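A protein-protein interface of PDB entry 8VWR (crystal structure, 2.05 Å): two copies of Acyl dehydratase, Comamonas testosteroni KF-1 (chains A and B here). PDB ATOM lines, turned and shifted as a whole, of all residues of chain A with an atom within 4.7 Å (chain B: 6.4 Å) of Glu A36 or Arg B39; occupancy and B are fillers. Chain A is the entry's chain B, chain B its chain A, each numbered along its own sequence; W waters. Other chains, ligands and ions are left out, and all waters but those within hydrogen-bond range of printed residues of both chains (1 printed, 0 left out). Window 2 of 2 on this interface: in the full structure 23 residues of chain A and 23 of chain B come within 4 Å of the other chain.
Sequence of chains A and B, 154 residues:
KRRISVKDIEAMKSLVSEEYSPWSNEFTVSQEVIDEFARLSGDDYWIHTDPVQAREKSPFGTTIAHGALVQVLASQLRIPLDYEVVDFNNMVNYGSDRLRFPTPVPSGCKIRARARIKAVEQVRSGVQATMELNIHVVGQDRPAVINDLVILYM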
ATOM      1  N   GLU A  32      30.729 -11.993  -5.604  1.00  0.00           N
ATOM      2  CA  GLU A  32      29.561 -11.434  -6.275  1.00  0.00           C
ATOM      3  C   GLU A  32      29.105 -12.334  -7.416  1.00  0.00           C
ATOM      4  O   GLU A  32      27.905 -12.579  -7.587  1.00  0.00           O
ATOM      5  CB  GLU A  32      29.879 -10.029  -6.790  1.00  0.00           C
ATOM      6  CG  GLU A  32      30.114  -8.988  -5.696  1.00  0.00           C
ATOM      7  CD  GLU A  32      31.467  -9.123  -5.010  1.00  0.00           C
ATOM      8  OE1 GLU A  32      32.363  -9.790  -5.568  1.00  0.00           O
ATOM      9  OE2 GLU A  32      31.631  -8.561  -3.908  1.00  0.00           O
ATOM     10  N   VAL A  33      30.053 -12.837  -8.207  1.00  0.00           N
ATOM     11  CA  VAL A  33      29.720 -13.778  -9.272  1.00  0.00           C
ATOM     12  C   VAL A  33      29.084 -15.034  -8.685  1.00  0.00           C
ATOM     13  O   VAL A  33      28.067 -15.530  -9.182  1.00  0.00           O
ATOM     14  CB  VAL A  33      30.974 -14.111 -10.099  1.00  0.00           C
ATOM     15  CG1 VAL A  33      30.741 -15.333 -10.964  1.00  0.00           C
ATOM     16  CG2 VAL A  33      31.376 -12.917 -10.959  1.00  0.00           C
ATOM     17  N   ILE A  34      29.675 -15.564  -7.610  1.00  0.00           N
ATOM     18  CA  ILE A  34      29.138 -16.775  -6.994  1.00  0.00           C
ATOM     19  C   ILE A  34      27.732 -16.525  -6.464  1.00  0.00           C
ATOM     20  O   ILE A  34      26.824 -17.344  -6.656  1.00  0.00           O
ATOM     21  CB  ILE A  34      30.086 -17.272  -5.885  1.00  0.00           C
ATOM     22  CG1 ILE A  34      31.441 -17.667  -6.482  1.00  0.00           C
ATOM     23  CG2 ILE A  34      29.458 -18.440  -5.137  1.00  0.00           C
ATOM     24  CD1 ILE A  34      32.535 -17.883  -5.447  1.00  0.00           C
ATOM     25  N   ASP A  35      27.526 -15.389  -5.793  1.00  0.00           N
ATOM     26  CA  ASP A  35      26.210 -15.079  -5.244  1.00  0.00           C
ATOM     27  C   ASP A  35      25.158 -14.977  -6.342  1.00  0.00           C
ATOM     28  O   ASP A  35      24.036 -15.473  -6.182  1.00  0.00           O
ATOM     29  CB  ASP A  35      26.271 -13.779  -4.441  1.00  0.00           C
ATOM     30  CG  ASP A  35      27.001 -13.940  -3.121  1.00  0.00           C
ATOM     31  OD1 ASP A  35      27.302 -15.093  -2.746  1.00  0.00           O
ATOM     32  OD2 ASP A  35      27.274 -12.917  -2.459  1.00  0.00           O
ATOM     33  N   GLU A  36      25.495 -14.333  -7.463  1.00  0.00           N
ATOM     34  CA  GLU A  36      24.529 -14.204  -8.549  1.00  0.00           C
ATOM     35  C   GLU A  36      24.168 -15.566  -9.131  1.00  0.00           C
ATOM     36  O   GLU A  36      22.995 -15.837  -9.415  1.00  0.00           O
ATOM     37  CB  GLU A  36      25.070 -13.295  -9.650  1.00  0.00           C
ATOM     38  CG  GLU A  36      24.061 -13.074 -10.770  1.00  0.00           C
ATOM     39  CD  GLU A  36      24.594 -12.225 -11.904  1.00  0.00           C
ATOM     40  OE1 GLU A  36      25.765 -11.793 -11.837  1.00  0.00           O
ATOM     41  OE2 GLU A  36      23.832 -11.992 -12.866  1.00  0.00           O
ATOM     42  N   PHE A  37      25.163 -16.428  -9.343  1.00  0.00           N
ATOM     43  CA  PHE A  37      24.860 -17.771  -9.830  1.00  0.00           C
ATOM     44  C   PHE A  37      23.949 -18.504  -8.853  1.00  0.00           C
ATOM     45  O   PHE A  37      23.058 -19.254  -9.267  1.00  0.00           O
ATOM     46  CB  PHE A  37      26.150 -18.554 -10.060  1.00  0.00           C
ATOM     47  CG  PHE A  37      25.930 -19.927 -10.627  1.00  0.00           C
ATOM     48  CD1 PHE A  37      25.825 -20.119 -11.996  1.00  0.00           C
ATOM     49  CD2 PHE A  37      25.831 -21.026  -9.791  1.00  0.00           C
ATOM     50  CE1 PHE A  37      25.624 -21.384 -12.520  1.00  0.00           C
ATOM     51  CE2 PHE A  37      25.627 -22.293 -10.309  1.00  0.00           C
ATOM     52  CZ  PHE A  37      25.526 -22.472 -11.677  1.00  0.00           C
ATOM     53  N   ALA A  38      24.151 -18.289  -7.549  1.00  0.00           N
ATOM     54  CA  ALA A  38      23.272 -18.903  -6.560  1.00  0.00           C
ATOM     55  C   ALA A  38      21.830 -18.457  -6.761  1.00  0.00           C
ATOM     56  O   ALA A  38      20.906 -19.278  -6.720  1.00  0.00           O
ATOM     57  CB  ALA A  38      23.744 -18.559  -5.147  1.00  0.00           C
ATOM     58  N   ARG A  39      21.617 -17.160  -6.987  1.00  0.00           N
ATOM     59  CA  ARG A  39      20.259 -16.660  -7.173  1.00  0.00           C
ATOM     60  C   ARG A  39      19.675 -17.129  -8.500  1.00  0.00           C
ATOM     61  O   ARG A  39      18.507 -17.529  -8.565  1.00  0.00           O
ATOM     62  CB  ARG A  39      20.248 -15.134  -7.086  1.00  0.00           C
ATOM     63  CG  ARG A  39      20.500 -14.580  -5.688  1.00  0.00           C
ATOM     64  CD  ARG A  39      20.456 -13.056  -5.672  1.00  0.00           C
ATOM     65  NE  ARG A  39      21.598 -12.464  -6.357  1.00  0.00           N
ATOM     66  CZ  ARG A  39      22.689 -12.007  -5.754  1.00  0.00           C
ATOM     67  NH1 ARG A  39      22.819 -12.039  -4.437  1.00  0.00           N
ATOM     68  NH2 ARG A  39      23.673 -11.501  -6.491  1.00  0.00           N
ATOM     69  N   LEU A  40      20.475 -17.096  -9.568  1.00  0.00           N
ATOM     70  CA  LEU A  40      19.979 -17.481 -10.886  1.00  0.00           C
ATOM     71  C   LEU A  40      19.619 -18.962 -10.928  1.00  0.00           C
ATOM     72  O   LEU A  40      18.523 -19.333 -11.365  1.00  0.00           O
ATOM     73  CB  LEU A  40      21.031 -17.145 -11.945  1.00  0.00           C
ATOM     74  CG  LEU A  40      20.670 -17.310 -13.421  1.00  0.00           C
ATOM     75  CD1 LEU A  40      21.651 -16.533 -14.296  1.00  0.00           C
ATOM     76  CD2 LEU A  40      20.670 -18.768 -13.829  1.00  0.00           C
ATOM     77  N   GLN A  76      33.874 -17.286 -20.800  1.00  0.00           N
ATOM     78  CA  GLN A  76      34.693 -16.107 -20.559  1.00  0.00           C
ATOM     79  C   GLN A  76      36.143 -16.307 -20.982  1.00  0.00           C
ATOM     80  O   GLN A  76      36.907 -15.334 -21.003  1.00  0.00           O
ATOM     81  CB  GLN A  76      34.666 -15.729 -19.072  1.00  0.00           C
ATOM     82  CG  GLN A  76      33.307 -15.326 -18.541  1.00  0.00           C
ATOM     83  CD  GLN A  76      32.904 -13.933 -18.971  1.00  0.00           C
ATOM     84  OE1 GLN A  76      33.682 -13.212 -19.596  1.00  0.00           O
ATOM     85  NE2 GLN A  76      31.683 -13.544 -18.634  1.00  0.00           N
ATOM     86  N   ILE B  34      17.563 -15.546 -19.700  1.00  0.00           N
ATOM     87  CA  ILE B  34      18.509 -15.889 -20.758  1.00  0.00           C
ATOM     88  C   ILE B  34      19.554 -14.790 -20.910  1.00  0.00           C
ATOM     89  O   ILE B  34      20.755 -15.062 -21.023  1.00  0.00           O
ATOM     90  CB  ILE B  34      17.755 -16.140 -22.078  1.00  0.00           C
ATOM     91  CG1 ILE B  34      16.803 -17.334 -21.928  1.00  0.00           C
ATOM     92  CG2 ILE B  34      18.724 -16.383 -23.227  1.00  0.00           C
ATOM     93  CD1 ILE B  34      15.835 -17.513 -23.086  1.00  0.00           C
ATOM     94  N   ASP B  35      19.112 -13.529 -20.917  1.00  0.00           N
ATOM     95  CA  ASP B  35      20.054 -12.429 -21.108  1.00  0.00           C
ATOM     96  C   ASP B  35      21.040 -12.340 -19.948  1.00  0.00           C
ATOM     97  O   ASP B  35      22.230 -12.080 -20.159  1.00  0.00           O
ATOM     98  CB  ASP B  35      19.299 -11.110 -21.275  1.00  0.00           C
ATOM     99  CG  ASP B  35      18.521 -11.043 -22.578  1.00  0.00           C
ATOM    100  OD1 ASP B  35      18.835 -11.822 -23.503  1.00  0.00           O
ATOM    101  OD2 ASP B  35      17.598 -10.208 -22.678  1.00  0.00           O
ATOM    102  N   GLU B  36      20.566 -12.556 -18.719  1.00  0.00           N
ATOM    103  CA  GLU B  36      21.463 -12.515 -17.570  1.00  0.00           C
ATOM    104  C   GLU B  36      22.501 -13.628 -17.646  1.00  0.00           C
ATOM    105  O   GLU B  36      23.685 -13.403 -17.369  1.00  0.00           O
ATOM    106  CB  GLU B  36      20.668 -12.624 -16.269  1.00  0.00           C
ATOM    107  CG  GLU B  36      21.532 -12.607 -15.015  1.00  0.00           C
ATOM    108  CD  GLU B  36      20.738 -12.887 -13.752  1.00  0.00           C
ATOM    109  OE1 GLU B  36      19.516 -13.118 -13.858  1.00  0.00           O
ATOM    110  OE2 GLU B  36      21.337 -12.878 -12.655  1.00  0.00           O
ATOM    111  N   PHE B  37      22.072 -14.839 -18.006  1.00  0.00           N
ATOM    112  CA  PHE B  37      23.021 -15.935 -18.159  1.00  0.00           C
ATOM    113  C   PHE B  37      24.032 -15.635 -19.259  1.00  0.00           C
ATOM    114  O   PHE B  37      25.202 -16.019 -19.160  1.00  0.00           O
ATOM    115  CB  PHE B  37      22.286 -17.242 -18.458  1.00  0.00           C
ATOM    116  CG  PHE B  37      23.200 -18.432 -18.595  1.00  0.00           C
ATOM    117  CD1 PHE B  37      23.560 -19.181 -17.485  1.00  0.00           C
ATOM    118  CD2 PHE B  37      23.702 -18.799 -19.833  1.00  0.00           C
ATOM    119  CE1 PHE B  37      24.403 -20.273 -17.610  1.00  0.00           C
ATOM    120  CE2 PHE B  37      24.544 -19.888 -19.962  1.00  0.00           C
ATOM    121  CZ  PHE B  37      24.895 -20.625 -18.848  1.00  0.00           C
ATOM    122  N   ALA B  38      23.596 -14.954 -20.325  1.00  0.00           N
ATOM    123  CA  ALA B  38      24.510 -14.638 -21.419  1.00  0.00           C
ATOM    124  C   ALA B  38      25.638 -13.730 -20.949  1.00  0.00           C
ATOM    125  O   ALA B  38      26.800 -13.921 -21.330  1.00  0.00           O
ATOM    126  CB  ALA B  38      23.744 -13.982 -22.569  1.00  0.00           C
ATOM    127  N   ARG B  39      25.315 -12.739 -20.117  1.00  0.00           N
ATOM    128  CA  ARG B  39      26.336 -11.823 -19.620  1.00  0.00           C
ATOM    129  C   ARG B  39      27.195 -12.478 -18.544  1.00  0.00           C
ATOM    130  O   ARG B  39      28.412 -12.264 -18.506  1.00  0.00           O
ATOM    131  CB  ARG B  39      25.675 -10.550 -19.083  1.00  0.00           C
ATOM    132  CG  ARG B  39      26.658  -9.481 -18.592  1.00  0.00           C
ATOM    133  CD  ARG B  39      26.930  -9.596 -17.094  1.00  0.00           C
ATOM    134  NE  ARG B  39      25.694  -9.550 -16.323  1.00  0.00           N
ATOM    135  CZ  ARG B  39      25.513 -10.144 -15.151  1.00  0.00           C
ATOM    136  NH1 ARG B  39      26.487 -10.817 -14.559  1.00  0.00           N
ATOM    137  NH2 ARG B  39      24.322 -10.072 -14.565  1.00  0.00           N
ATOM    138  N   LEU B  40      26.585 -13.272 -17.664  1.00  0.00           N
ATOM    139  CA  LEU B  40      27.349 -13.949 -16.620  1.00  0.00           C
ATOM    140  C   LEU B  40      28.331 -14.946 -17.224  1.00  0.00           C
ATOM    141  O   LEU B  40      29.499 -15.010 -16.820  1.00  0.00           O
ATOM    142  CB  LEU B  40      26.397 -14.651 -15.649  1.00  0.00           C
ATOM    143  CG  LEU B  40      26.989 -15.210 -14.353  1.00  0.00           C
ATOM    144  CD1 LEU B  40      25.907 -15.361 -13.293  1.00  0.00           C
ATOM    145  CD2 LEU B  40      27.676 -16.547 -14.573  1.00  0.00           C
ATOM    146  N   SER B  41      27.873 -15.736 -18.197  1.00  0.00           N
ATOM    147  CA  SER B  41      28.721 -16.769 -18.775  1.00  0.00           C
ATOM    148  C   SER B  41      29.651 -16.225 -19.851  1.00  0.00           C
ATOM    149  O   SER B  41      30.735 -16.778 -20.060  1.00  0.00           O
ATOM    150  CB  SER B  41      27.859 -17.885 -19.368  1.00  0.00           C
ATOM    151  OG  SER B  41      27.144 -17.427 -20.503  1.00  0.00           O
ATOM    152  N   GLY B  42      29.254 -15.156 -20.539  1.00  0.00           N
ATOM    153  CA  GLY B  42      29.979 -14.678 -21.693  1.00  0.00           C
ATOM    154  C   GLY B  42      29.461 -15.194 -23.019  1.00  0.00           C
ATOM    155  O   GLY B  42      29.923 -14.732 -24.070  1.00  0.00           O
ATOM    156  N   ASP B  43      28.513 -16.125 -23.006  1.00  0.00           N
ATOM    157  CA  ASP B  43      27.961 -16.705 -24.230  1.00  0.00           C
ATOM    158  C   ASP B  43      26.751 -15.876 -24.645  1.00  0.00           C
ATOM    159  O   ASP B  43      25.646 -16.071 -24.135  1.00  0.00           O
ATOM    160  CB  ASP B  43      27.595 -18.166 -23.996  1.00  0.00           C
ATOM    161  CG  ASP B  43      27.019 -18.832 -25.228  1.00  0.00           C
ATOM    162  OD1 ASP B  43      26.968 -18.187 -26.297  1.00  0.00           O
ATOM    163  OD2 ASP B  43      26.616 -20.011 -25.123  1.00  0.00           O
ATOM    164  N   ASP B  44      26.955 -14.945 -25.580  1.00  0.00           N
ATOM    165  CA  ASP B  44      25.891 -14.064 -26.049  1.00  0.00           C
ATOM    166  C   ASP B  44      25.501 -14.351 -27.500  1.00  0.00           C
ATOM    167  O   ASP B  44      25.081 -13.450 -28.230  1.00  0.00           O
ATOM    168  CB  ASP B  44      26.299 -12.600 -25.882  1.00  0.00           C
ATOM    169  CG  ASP B  44      27.468 -12.212 -26.763  1.00  0.00           C
ATOM    170  OD1 ASP B  44      28.236 -13.108 -27.172  1.00  0.00           O
ATOM    171  OD2 ASP B  44      27.622 -11.004 -27.042  1.00  0.00           O
HETATM  172  O   HOH W   1      30.154 -11.060 -20.095  1.00  0.00           O
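The backbone carbonyl oxygen of Ser B41 sits at hydrogen-bond distance from the backbone NH of Gln A76 (3.3 Å). The guanidinium group (NH2) of Arg B39 is in salt-bridge range of the side-chain carboxylate (OE2) of Glu A36 (2.6 Å). The side-chain carboxylate of Glu B36 sits close to the side-chain carboxylate of Glu A36, 2.7 Å away. The backbone carbonyl oxygen (O) of Leu B40 lies within hydrogen-bond range of the side-chain amide nitrogen (NE2) of Gln A76, at 3.2 Å. The backbone NH (N) of Gly B42 sits close to the side-chain amide nitrogen (NE2) of Gln A76 (3.5 Å).
The side-chain hydroxyl (OG) of Ser B41 lies within hydrogen-bond range of the backbone carbonyl oxygen (O) of Phe B37, 2.7 Å away. N of Asp B43 lies within hydrogen-bond range of OG of Ser B41 (3.1 Å).
Glu A36 touches Leu B40. Leu A40 touches Glu B36. Gln A76 touches Arg B39 (NE2 to O, 3.5 Å).
Of the printed residues of chain B, Glu A36 touches Glu B36, Arg B39 and Leu B40. Ala A38 touches none of the printed residues of chain B. Printed residues of chain B within 4 Å of Gln A76: Arg B39, Leu B40, Ser B41 and Gly B42. Of the printed residues of chain A, Glu B36 touches Glu A36 (2.7 Å) and Leu A40 (3.8 Å). Phe B37 touches none of the printed residues of chain A. Of chain A, only Glu A36 and Gln A76 come within 4 Å of Arg B39. The nearest residue of chain B that does not touch Glu A36 is Phe B37 (6.1 Å). The nearest printed residue of chain A that does not touch Arg B39 is Val A33 (6.4 Å). The nearest printed residue of chain A that does not touch Gly B42 is Val A33 (9.7 Å).
Hydrophobic or aromatic side chains of chain A within 4 Å of the printed part of chain B: Leu A40. Among the printed residues, 8 pairs touch across the chains. Among the printed residues, Asp or Glu carboxylates within 4 Å of a Lys or Arg side-chain nitrogen of the other chain: Glu A36 with Arg B39 (2.6 Å).
Glu A36 touches its own counterpart, Glu B36. Glu A36 touches Arg B39, but with the chains exchanged Arg A39 does not touch Glu B36 (6.1 Å). Glu A36 touches Leu B40, and with the chains exchanged Leu A40 touches Glu B36. Of the 8 pairs that touch across the chains among the printed residues, 3 have their exchanged pair printed and touching as well.
Water W1 lies within hydrogen-bond range of the backbone carbonyl oxygen of Arg B39 (2.6 Å) and the side-chain amide nitrogen of Gln A76 (3.3 Å).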
